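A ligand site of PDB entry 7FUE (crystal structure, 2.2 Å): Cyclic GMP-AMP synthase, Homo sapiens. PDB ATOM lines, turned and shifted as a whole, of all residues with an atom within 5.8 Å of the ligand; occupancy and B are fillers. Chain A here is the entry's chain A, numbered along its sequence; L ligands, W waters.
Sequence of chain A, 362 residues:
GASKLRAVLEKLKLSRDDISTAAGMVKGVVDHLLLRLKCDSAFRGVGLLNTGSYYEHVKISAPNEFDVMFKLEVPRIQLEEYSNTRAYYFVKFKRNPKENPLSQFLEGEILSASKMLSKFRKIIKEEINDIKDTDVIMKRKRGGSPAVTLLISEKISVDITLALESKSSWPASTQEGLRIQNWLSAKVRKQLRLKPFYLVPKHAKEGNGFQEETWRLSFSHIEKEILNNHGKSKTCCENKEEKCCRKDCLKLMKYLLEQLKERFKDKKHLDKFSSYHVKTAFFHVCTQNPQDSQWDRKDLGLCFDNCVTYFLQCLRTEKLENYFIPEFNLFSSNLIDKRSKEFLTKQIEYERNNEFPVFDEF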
ATOM      1  N   ARG A  86     -31.594  21.290  -5.049  1.00  0.00           N
ATOM      2  CA  ARG A  86     -30.167  21.018  -5.067  1.00  0.00           C
ATOM      3  C   ARG A  86     -29.405  21.768  -6.157  1.00  0.00           C
ATOM      4  O   ARG A  86     -28.207  22.048  -5.984  1.00  0.00           O
ATOM      5  CB  ARG A  86     -29.912  19.510  -5.202  1.00  0.00           C
ATOM      6  CG  ARG A  86     -30.284  18.717  -3.967  1.00  0.00           C
ATOM      7  CD  ARG A  86     -29.546  19.219  -2.714  1.00  0.00           C
ATOM      8  NE  ARG A  86     -29.860  18.390  -1.557  1.00  0.00           N
ATOM      9  CZ  ARG A  86     -30.846  18.622  -0.694  1.00  0.00           C
ATOM     10  NH1 ARG A  86     -31.048  17.801   0.334  1.00  0.00           N
ATOM     11  NH2 ARG A  86     -31.648  19.681  -0.833  1.00  0.00           N
ATOM     12  N   ALA A  87     -30.076  22.144  -7.259  1.00  0.00           N
ATOM     13  CA  ALA A  87     -29.396  22.703  -8.423  1.00  0.00           C
ATOM     14  C   ALA A  87     -29.840  24.111  -8.818  1.00  0.00           C
ATOM     15  O   ALA A  87     -29.144  24.756  -9.623  1.00  0.00           O
ATOM     16  CB  ALA A  87     -29.588  21.780  -9.639  1.00  0.00           C
ATOM     17  N   TYR A  88     -30.964  24.588  -8.302  1.00  0.00           N
ATOM     18  CA  TYR A  88     -31.536  25.871  -8.679  1.00  0.00           C
ATOM     19  C   TYR A  88     -31.488  26.823  -7.489  1.00  0.00           C
ATOM     20  O   TYR A  88     -31.834  26.443  -6.367  1.00  0.00           O
ATOM     21  CB  TYR A  88     -32.969  25.684  -9.188  1.00  0.00           C
ATOM     22  CG  TYR A  88     -33.029  24.887 -10.496  1.00  0.00           C
ATOM     23  CD1 TYR A  88     -32.833  25.512 -11.732  1.00  0.00           C
ATOM     24  CD2 TYR A  88     -33.288  23.516 -10.496  1.00  0.00           C
ATOM     25  CE1 TYR A  88     -32.879  24.803 -12.924  1.00  0.00           C
ATOM     26  CE2 TYR A  88     -33.332  22.787 -11.690  1.00  0.00           C
ATOM     27  CZ  TYR A  88     -33.120  23.430 -12.898  1.00  0.00           C
ATOM     28  OH  TYR A  88     -33.178  22.718 -14.074  1.00  0.00           O
ATOM     29  N   LEU A 178     -18.167  15.040  -8.440  1.00  0.00           N
ATOM     30  CA  LEU A 178     -16.869  14.980  -9.084  1.00  0.00           C
ATOM     31  C   LEU A 178     -16.057  13.817  -8.527  1.00  0.00           C
ATOM     32  O   LEU A 178     -14.939  13.959  -8.049  1.00  0.00           O
ATOM     33  CB  LEU A 178     -16.164  16.331  -8.929  1.00  0.00           C
ATOM     34  CG  LEU A 178     -15.014  16.653  -9.888  1.00  0.00           C
ATOM     35  CD1 LEU A 178     -15.506  16.614 -11.331  1.00  0.00           C
ATOM     36  CD2 LEU A 178     -14.409  18.004  -9.567  1.00  0.00           C
ATOM     37  N   ARG A 216     -29.187  28.202 -12.314  1.00  0.00           N
ATOM     38  CA  ARG A 216     -28.769  26.807 -12.265  1.00  0.00           C
ATOM     39  C   ARG A 216     -27.243  26.729 -12.297  1.00  0.00           C
ATOM     40  O   ARG A 216     -26.615  27.399 -13.110  1.00  0.00           O
ATOM     41  CB  ARG A 216     -29.380  26.033 -13.439  1.00  0.00           C
ATOM     42  CG  ARG A 216     -28.853  24.606 -13.619  1.00  0.00           C
ATOM     43  CD  ARG A 216     -29.399  23.868 -14.862  1.00  0.00           C
ATOM     44  NE  ARG A 216     -29.006  24.476 -16.144  1.00  0.00           N
ATOM     45  CZ  ARG A 216     -27.766  24.491 -16.627  1.00  0.00           C
ATOM     46  NH1 ARG A 216     -26.742  23.952 -15.963  1.00  0.00           N
ATOM     47  NH2 ARG A 216     -27.536  25.062 -17.810  1.00  0.00           N
ATOM     48  N   LEU A 217     -26.649  25.900 -11.431  1.00  0.00           N
ATOM     49  CA  LEU A 217     -25.195  25.767 -11.402  1.00  0.00           C
ATOM     50  C   LEU A 217     -24.708  25.162 -12.703  1.00  0.00           C
ATOM     51  O   LEU A 217     -25.274  24.171 -13.189  1.00  0.00           O
ATOM     52  CB  LEU A 217     -24.755  24.877 -10.247  1.00  0.00           C
ATOM     53  CG  LEU A 217     -25.094  25.319  -8.829  1.00  0.00           C
ATOM     54  CD1 LEU A 217     -24.636  24.241  -7.850  1.00  0.00           C
ATOM     55  CD2 LEU A 217     -24.400  26.629  -8.526  1.00  0.00           C
ATOM     56  N   SER A 218     -23.640  25.729 -13.269  1.00  0.00           N
ATOM     57  CA  SER A 218     -23.056  25.244 -14.498  1.00  0.00           C
ATOM     58  C   SER A 218     -21.581  24.957 -14.281  1.00  0.00           C
ATOM     59  O   SER A 218     -20.849  25.820 -13.784  1.00  0.00           O
ATOM     60  CB  SER A 218     -23.220  26.269 -15.634  1.00  0.00           C
ATOM     61  OG  SER A 218     -22.563  25.835 -16.811  1.00  0.00           O
ATOM     62  N   PHE A 219     -21.143  23.770 -14.657  1.00  0.00           N
ATOM     63  CA  PHE A 219     -19.720  23.443 -14.638  1.00  0.00           C
ATOM     64  C   PHE A 219     -19.211  23.097 -16.049  1.00  0.00           C
ATOM     65  O   PHE A 219     -18.472  22.147 -16.240  1.00  0.00           O
ATOM     66  CB  PHE A 219     -19.435  22.309 -13.662  1.00  0.00           C
ATOM     67  CG  PHE A 219     -19.887  22.581 -12.261  1.00  0.00           C
ATOM     68  CD1 PHE A 219     -19.068  23.260 -11.381  1.00  0.00           C
ATOM     69  CD2 PHE A 219     -21.128  22.187 -11.830  1.00  0.00           C
ATOM     70  CE1 PHE A 219     -19.464  23.523 -10.105  1.00  0.00           C
ATOM     71  CE2 PHE A 219     -21.541  22.435 -10.531  1.00  0.00           C
ATOM     72  CZ  PHE A 219     -20.703  23.110  -9.676  1.00  0.00           C
ATOM     73  N   SER A 220     -19.659  23.874 -17.043  1.00  0.00           N
ATOM     74  CA  SER A 220     -19.198  23.803 -18.422  1.00  0.00           C
ATOM     75  C   SER A 220     -17.696  23.548 -18.507  1.00  0.00           C
ATOM     76  O   SER A 220     -17.227  22.553 -19.088  1.00  0.00           O
ATOM     77  CB  SER A 220     -19.498  25.126 -19.144  1.00  0.00           C
ATOM     78  OG  SER A 220     -20.739  25.098 -19.806  1.00  0.00           O
ATOM     79  N   HIS A 221     -16.953  24.449 -17.907  1.00  0.00           N
ATOM     80  CA  HIS A 221     -15.512  24.583 -18.074  1.00  0.00           C
ATOM     81  C   HIS A 221     -14.738  23.383 -17.566  1.00  0.00           C
ATOM     82  O   HIS A 221     -13.552  23.286 -17.845  1.00  0.00           O
ATOM     83  CB  HIS A 221     -15.046  25.816 -17.337  1.00  0.00           C
ATOM     84  CG  HIS A 221     -15.389  25.817 -15.883  1.00  0.00           C
ATOM     85  ND1 HIS A 221     -16.574  25.328 -15.377  1.00  0.00           N
ATOM     86  CD2 HIS A 221     -14.708  26.296 -14.805  1.00  0.00           C
ATOM     87  CE1 HIS A 221     -16.594  25.480 -14.069  1.00  0.00           C
ATOM     88  NE2 HIS A 221     -15.474  26.070 -13.689  1.00  0.00           N
ATOM     89  N   ILE A 222     -15.382  22.471 -16.851  1.00  0.00           N
ATOM     90  CA  ILE A 222     -14.649  21.357 -16.255  1.00  0.00           C
ATOM     91  C   ILE A 222     -14.385  20.249 -17.280  1.00  0.00           C
ATOM     92  O   ILE A 222     -13.416  19.500 -17.143  1.00  0.00           O
ATOM     93  CB  ILE A 222     -15.428  20.835 -15.057  1.00  0.00           C
ATOM     94  CG1 ILE A 222     -15.517  21.936 -14.016  1.00  0.00           C
ATOM     95  CG2 ILE A 222     -14.736  19.627 -14.473  1.00  0.00           C
ATOM     96  CD1 ILE A 222     -14.204  22.286 -13.363  1.00  0.00           C
ATOM     97  N   GLU A 223     -15.255  20.120 -18.304  1.00  0.00           N
ATOM     98  CA  GLU A 223     -15.100  19.060 -19.300  1.00  0.00           C
ATOM     99  C   GLU A 223     -13.786  19.187 -20.047  1.00  0.00           C
ATOM    100  O   GLU A 223     -13.040  18.212 -20.199  1.00  0.00           O
ATOM    101  CB  GLU A 223     -16.264  19.093 -20.297  1.00  0.00           C
ATOM    102  CG  GLU A 223     -16.170  18.101 -21.478  1.00  0.00           C
ATOM    103  CD  GLU A 223     -17.338  18.245 -22.469  1.00  0.00           C
ATOM    104  OE1 GLU A 223     -17.961  19.323 -22.481  1.00  0.00           O
ATOM    105  OE2 GLU A 223     -17.626  17.297 -23.243  1.00  0.00           O
ATOM    106  N   ILE A 226     -10.949  17.994 -17.906  1.00  0.00           N
ATOM    107  CA  ILE A 226     -10.791  16.556 -17.795  1.00  0.00           C
ATOM    108  C   ILE A 226     -10.381  15.958 -19.127  1.00  0.00           C
ATOM    109  O   ILE A 226      -9.411  15.197 -19.208  1.00  0.00           O
ATOM    110  CB  ILE A 226     -12.055  15.941 -17.235  1.00  0.00           C
ATOM    111  CG1 ILE A 226     -12.266  16.498 -15.836  1.00  0.00           C
ATOM    112  CG2 ILE A 226     -11.934  14.434 -17.242  1.00  0.00           C
ATOM    113  CD1 ILE A 226     -13.269  15.691 -15.093  1.00  0.00           C
ATOM    114  N   SER A 274     -30.312  15.440 -24.478  1.00  0.00           N
ATOM    115  CA  SER A 274     -29.277  16.234 -25.099  1.00  0.00           C
ATOM    116  C   SER A 274     -27.926  15.640 -24.720  1.00  0.00           C
ATOM    117  O   SER A 274     -27.854  14.684 -23.943  1.00  0.00           O
ATOM    118  CB  SER A 274     -29.387  17.697 -24.674  1.00  0.00           C
ATOM    119  OG  SER A 274     -29.176  17.789 -23.291  1.00  0.00           O
ATOM    120  N   TYR A 276     -25.605  16.580 -22.757  1.00  0.00           N
ATOM    121  CA  TYR A 276     -25.088  16.488 -21.383  1.00  0.00           C
ATOM    122  C   TYR A 276     -25.560  15.211 -20.700  1.00  0.00           C
ATOM    123  O   TYR A 276     -24.881  14.692 -19.811  1.00  0.00           O
ATOM    124  CB  TYR A 276     -25.430  17.728 -20.569  1.00  0.00           C
ATOM    125  CG  TYR A 276     -26.835  17.849 -20.082  1.00  0.00           C
ATOM    126  CD1 TYR A 276     -27.194  17.358 -18.827  1.00  0.00           C
ATOM    127  CD2 TYR A 276     -27.796  18.506 -20.827  1.00  0.00           C
ATOM    128  CE1 TYR A 276     -28.508  17.498 -18.344  1.00  0.00           C
ATOM    129  CE2 TYR A 276     -29.113  18.657 -20.357  1.00  0.00           C
ATOM    130  CZ  TYR A 276     -29.465  18.148 -19.113  1.00  0.00           C
ATOM    131  OH  TYR A 276     -30.764  18.304 -18.666  1.00  0.00           O
ATOM    132  N   LYS A 279     -22.807  13.019 -21.981  1.00  0.00           N
ATOM    133  CA  LYS A 279     -21.564  13.355 -21.268  1.00  0.00           C
ATOM    134  C   LYS A 279     -21.587  12.794 -19.863  1.00  0.00           C
ATOM    135  O   LYS A 279     -20.656  12.068 -19.459  1.00  0.00           O
ATOM    136  CB  LYS A 279     -21.372  14.874 -21.212  1.00  0.00           C
ATOM    137  CG  LYS A 279     -21.090  15.473 -22.580  1.00  0.00           C
ATOM    138  CD  LYS A 279     -20.781  16.974 -22.528  1.00  0.00           C
ATOM    139  CE  LYS A 279     -20.760  17.508 -23.966  1.00  0.00           C
ATOM    140  NZ  LYS A 279     -20.154  18.844 -24.078  1.00  0.00           N
ATOM    141  N   THR A 280     -22.658  13.092 -19.102  1.00  0.00           N
ATOM    142  CA  THR A 280     -22.788  12.608 -17.737  1.00  0.00           C
ATOM    143  C   THR A 280     -22.597  11.096 -17.654  1.00  0.00           C
ATOM    144  O   THR A 280     -21.816  10.597 -16.849  1.00  0.00           O
ATOM    145  CB  THR A 280     -24.169  12.935 -17.178  1.00  0.00           C
ATOM    146  OG1 THR A 280     -24.352  14.357 -17.107  1.00  0.00           O
ATOM    147  CG2 THR A 280     -24.267  12.380 -15.790  1.00  0.00           C
ATOM    148  N   PHE A 283     -18.987  10.007 -18.169  1.00  0.00           N
ATOM    149  CA  PHE A 283     -18.013  10.220 -17.100  1.00  0.00           C
ATOM    150  C   PHE A 283     -18.271   9.295 -15.933  1.00  0.00           C
ATOM    151  O   PHE A 283     -17.338   8.996 -15.163  1.00  0.00           O
ATOM    152  CB  PHE A 283     -17.974  11.679 -16.690  1.00  0.00           C
ATOM    153  CG  PHE A 283     -17.270  12.552 -17.685  1.00  0.00           C
ATOM    154  CD1 PHE A 283     -15.899  12.441 -17.878  1.00  0.00           C
ATOM    155  CD2 PHE A 283     -17.964  13.444 -18.485  1.00  0.00           C
ATOM    156  CE1 PHE A 283     -15.220  13.204 -18.824  1.00  0.00           C
ATOM    157  CE2 PHE A 283     -17.293  14.235 -19.420  1.00  0.00           C
ATOM    158  CZ  PHE A 283     -15.925  14.110 -19.592  1.00  0.00           C
ATOM    159  N   ASN A 322     -26.553  13.499 -11.862  1.00  0.00           N
ATOM    160  CA  ASN A 322     -25.678  14.585 -12.266  1.00  0.00           C
ATOM    161  C   ASN A 322     -24.279  14.348 -11.716  1.00  0.00           C
ATOM    162  O   ASN A 322     -24.119  13.881 -10.585  1.00  0.00           O
ATOM    163  CB  ASN A 322     -26.205  15.915 -11.738  1.00  0.00           C
ATOM    164  CG  ASN A 322     -25.314  17.061 -12.130  1.00  0.00           C
ATOM    165  OD1 ASN A 322     -24.317  17.359 -11.458  1.00  0.00           O
ATOM    166  ND2 ASN A 322     -25.644  17.671 -13.234  1.00  0.00           N
ATOM    167  N   TYR A 323     -23.253  14.678 -12.512  1.00  0.00           N
ATOM    168  CA  TYR A 323     -21.889  14.288 -12.132  1.00  0.00           C
ATOM    169  C   TYR A 323     -21.360  15.128 -10.982  1.00  0.00           C
ATOM    170  O   TYR A 323     -20.458  14.671 -10.254  1.00  0.00           O
ATOM    171  CB  TYR A 323     -20.939  14.422 -13.342  1.00  0.00           C
ATOM    172  CG  TYR A 323     -19.680  13.587 -13.194  1.00  0.00           C
ATOM    173  CD1 TYR A 323     -19.767  12.216 -13.306  1.00  0.00           C
ATOM    174  CD2 TYR A 323     -18.431  14.165 -12.936  1.00  0.00           C
ATOM    175  CE1 TYR A 323     -18.663  11.419 -13.166  1.00  0.00           C
ATOM    176  CE2 TYR A 323     -17.304  13.358 -12.793  1.00  0.00           C
ATOM    177  CZ  TYR A 323     -17.442  11.975 -12.920  1.00  0.00           C
ATOM    178  OH  TYR A 323     -16.392  11.105 -12.810  1.00  0.00           O
ATOM    179  N   PHE A 324     -21.891  16.331 -10.799  1.00  0.00           N
ATOM    180  CA  PHE A 324     -21.425  17.264  -9.779  1.00  0.00           C
ATOM    181  C   PHE A 324     -22.305  17.305  -8.544  1.00  0.00           C
ATOM    182  O   PHE A 324     -21.833  17.682  -7.454  1.00  0.00           O
ATOM    183  CB  PHE A 324     -21.342  18.674 -10.360  1.00  0.00           C
ATOM    184  CG  PHE A 324     -20.363  18.779 -11.478  1.00  0.00           C
ATOM    185  CD1 PHE A 324     -19.069  19.200 -11.231  1.00  0.00           C
ATOM    186  CD2 PHE A 324     -20.716  18.450 -12.774  1.00  0.00           C
ATOM    187  CE1 PHE A 324     -18.154  19.267 -12.264  1.00  0.00           C
ATOM    188  CE2 PHE A 324     -19.799  18.507 -13.809  1.00  0.00           C
ATOM    189  CZ  PHE A 324     -18.509  18.915 -13.541  1.00  0.00           C
ATOM    190  N   ILE A 325     -23.572  16.947  -8.709  1.00  0.00           N
ATOM    191  CA  ILE A 325     -24.593  17.061  -7.668  1.00  0.00           C
ATOM    192  C   ILE A 325     -25.325  15.724  -7.638  1.00  0.00           C
ATOM    193  O   ILE A 325     -26.356  15.553  -8.297  1.00  0.00           O
ATOM    194  CB  ILE A 325     -25.523  18.240  -7.968  1.00  0.00           C
ATOM    195  CG1 ILE A 325     -24.680  19.511  -8.030  1.00  0.00           C
ATOM    196  CG2 ILE A 325     -26.678  18.375  -6.948  1.00  0.00           C
ATOM    197  CD1 ILE A 325     -25.398  20.677  -8.630  1.00  0.00           C
ATOM    198  N   PHE A 328     -29.147  14.788  -7.739  1.00  0.00           N
ATOM    199  CA  PHE A 328     -30.022  15.223  -8.818  1.00  0.00           C
ATOM    200  C   PHE A 328     -30.033  14.137  -9.893  1.00  0.00           C
ATOM    201  O   PHE A 328     -28.995  13.825 -10.493  1.00  0.00           O
ATOM    202  CB  PHE A 328     -29.547  16.564  -9.371  1.00  0.00           C
ATOM    203  CG  PHE A 328     -30.555  17.233 -10.238  1.00  0.00           C
ATOM    204  CD1 PHE A 328     -31.319  18.263  -9.746  1.00  0.00           C
ATOM    205  CD2 PHE A 328     -30.756  16.817 -11.538  1.00  0.00           C
ATOM    206  CE1 PHE A 328     -32.256  18.898 -10.541  1.00  0.00           C
ATOM    207  CE2 PHE A 328     -31.685  17.434 -12.344  1.00  0.00           C
ATOM    208  CZ  PHE A 328     -32.435  18.484 -11.837  1.00  0.00           C
ATOM    209  N   LEU A 330     -31.074  13.220 -13.373  1.00  0.00           N
ATOM    210  CA  LEU A 330     -31.446  13.762 -14.687  1.00  0.00           C
ATOM    211  C   LEU A 330     -32.554  12.967 -15.351  1.00  0.00           C
ATOM    212  O   LEU A 330     -33.200  13.465 -16.284  1.00  0.00           O
ATOM    213  CB  LEU A 330     -30.202  13.821 -15.575  1.00  0.00           C
ATOM    214  CG  LEU A 330     -29.037  14.633 -15.004  1.00  0.00           C
ATOM    215  CD1 LEU A 330     -27.743  14.525 -15.826  1.00  0.00           C
ATOM    216  CD2 LEU A 330     -29.473  16.082 -14.928  1.00  0.00           C
HETATM  217  C1  LIG L   1     -22.229  18.285 -17.384  1.00  0.00           C
HETATM  218  C2  LIG L   1     -27.025  20.859 -14.499  1.00  0.00           C
HETATM  219  C3  LIG L   1     -28.231  20.581 -15.160  1.00  0.00           C
HETATM  220  C4  LIG L   1     -29.228  19.903 -14.474  1.00  0.00           C
HETATM  221  C5  LIG L   1     -29.030  19.489 -13.177  1.00  0.00           C
HETATM  222  C6  LIG L   1     -27.827  19.770 -12.544  1.00  0.00           C
HETATM  223  C7  LIG L   1     -28.431  21.018 -16.554  1.00  0.00           C
HETATM  224  C8  LIG L   1     -29.612  21.431 -17.210  1.00  0.00           C
HETATM  225  C9  LIG L   1     -29.242  21.742 -18.480  1.00  0.00           C
HETATM  226  C10 LIG L   1     -27.037  21.711 -19.715  1.00  0.00           C
HETATM  227  C11 LIG L   1     -21.103  16.001 -17.170  1.00  0.00           C
HETATM  228  C12 LIG L   1     -19.657  16.409 -17.026  1.00  0.00           C
HETATM  229  C13 LIG L   1     -26.796  20.454 -13.177  1.00  0.00           C
HETATM  230  C14 LIG L   1     -23.322  19.440 -15.606  1.00  0.00           C
HETATM  231  C15 LIG L   1     -21.972  16.951 -18.003  1.00  0.00           C
HETATM  232  C16 LIG L   1     -25.470  20.748 -12.474  1.00  0.00           C
HETATM  233  C17 LIG L   1     -19.196  17.629 -17.512  1.00  0.00           C
HETATM  234  C18 LIG L   1     -17.859  17.995 -17.356  1.00  0.00           C
HETATM  235  C19 LIG L   1     -16.978  17.152 -16.721  1.00  0.00           C
HETATM  236  C20 LIG L   1     -17.418  15.944 -16.230  1.00  0.00           C
HETATM  237  C21 LIG L   1     -18.747  15.578 -16.379  1.00  0.00           C
HETATM  238  C22 LIG L   1     -23.963  20.987 -14.410  1.00  0.00           C
HETATM  239  C23 LIG L   1     -22.017  20.735 -17.229  1.00  0.00           C
HETATM  240  C24 LIG L   1     -21.741  19.475 -17.856  1.00  0.00           C
HETATM  241  N1  LIG L   1     -23.018  18.279 -16.269  1.00  0.00           N
HETATM  242  N2  LIG L   1     -24.047  19.630 -14.542  1.00  0.00           N
HETATM  243  N3  LIG L   1     -27.908  21.521 -18.558  1.00  0.00           N
HETATM  244  N4  LIG L   1     -27.381  21.073 -17.400  1.00  0.00           N
HETATM  245  N5  LIG L   1     -24.635  21.556 -13.345  1.00  0.00           N
HETATM  246  N6  LIG L   1     -23.250  21.645 -15.301  1.00  0.00           N
HETATM  247  N7  LIG L   1     -22.834  20.603 -16.096  1.00  0.00           N
HETATM  248  O1  LIG L   1     -21.618  21.831 -17.584  1.00  0.00           O
HETATM  249 CL1  LIG L   1     -27.620  19.231 -10.911  1.00  0.00          CL
HETATM  250  O   HOH W   1     -23.681  15.810 -15.043  1.00  0.00           O
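The backbone carbonyl oxygen (O) of Leu 217 lies within hydrogen-bond range of a nitrogen (N5) of the ligand, at 2.7 Å.
The side-chain amide nitrogen (ND2) of Asn 322 is in hydrogen-bond range of a nitrogen (N2) of the ligand (2.8 Å).
O1 of the ligand is in hydrogen-bond range of N of Ser 220 (2.9 Å).
The backbone NH (N) of Phe 219 is in hydrogen-bond range of a nitrogen (N6) of the ligand (3.1 Å).
The guanidinium group of Arg 216 sits at hydrogen-bond distance from a nitrogen (N4) of the ligand (3.3 Å).
N of Leu 217 is in hydrogen-bond range of O of Ala 87 (3.3 Å).
The backbone NH (N) of Asn 322 is in hydrogen-bond range of the backbone carbonyl oxygen (O) of Phe 328 (2.8 Å).
The side-chain amide oxygen (OD1) of Asn 322 lies within hydrogen-bond range of the backbone NH (N) of Ile 325, 2.9 Å away.
OD1 of Asn 322 is in hydrogen-bond range of N of Phe 324 (2.7 Å).
The backbone carbonyl oxygen (O) of Phe 283 lies within hydrogen-bond range of the side-chain hydroxyl (OH) of Tyr 323, 3.3 Å away.
The backbone carbonyl oxygen of Tyr 276 sits at hydrogen-bond distance from the side-chain hydroxyl of Thr 280 (2.8 Å).
The side-chain carboxylate of Glu 223 is in salt-bridge range of the side-chain amino group of Lys 279 (2.8 Å).
The backbone carbonyl oxygen (O) of Tyr 323 is in hydrogen-bond range of the backbone NH (N) of Leu 178 (2.9 Å).
Merely in contact with the ligand: Ala 87 (3.5 Å), Ser 218 (3.7 Å), Glu 223 (3.5 Å), Tyr 276 (3.5 Å), Lys 279 (3.9 Å), Thr 280 (3.6 Å), Phe 283 (3.1 Å), Tyr 323 (3.7 Å), Phe 324 (3.8 Å), Ile 325 (3.5 Å), Phe 328 (3.5 Å) and Leu 330 (3.9 Å).
Hydrophobic or aromatic side chains within 4 Å of the ligand: Ala 87, Phe 219, Tyr 276, Phe 283, Tyr 323, Phe 324, Ile 325, Phe 328 and Leu 330.
17 residues have an atom within 4 Å of the ligand: Ala 87, Arg 216, Leu 217, Ser 218, Phe 219, Ser 220, Glu 223, Tyr 276, Lys 279, Thr 280, Phe 283, Asn 322, Tyr 323, Phe 324, Ile 325, Phe 328 and Leu 330.
Along chain A the residues within 4 Å of the ligand span positions 87 to 330.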
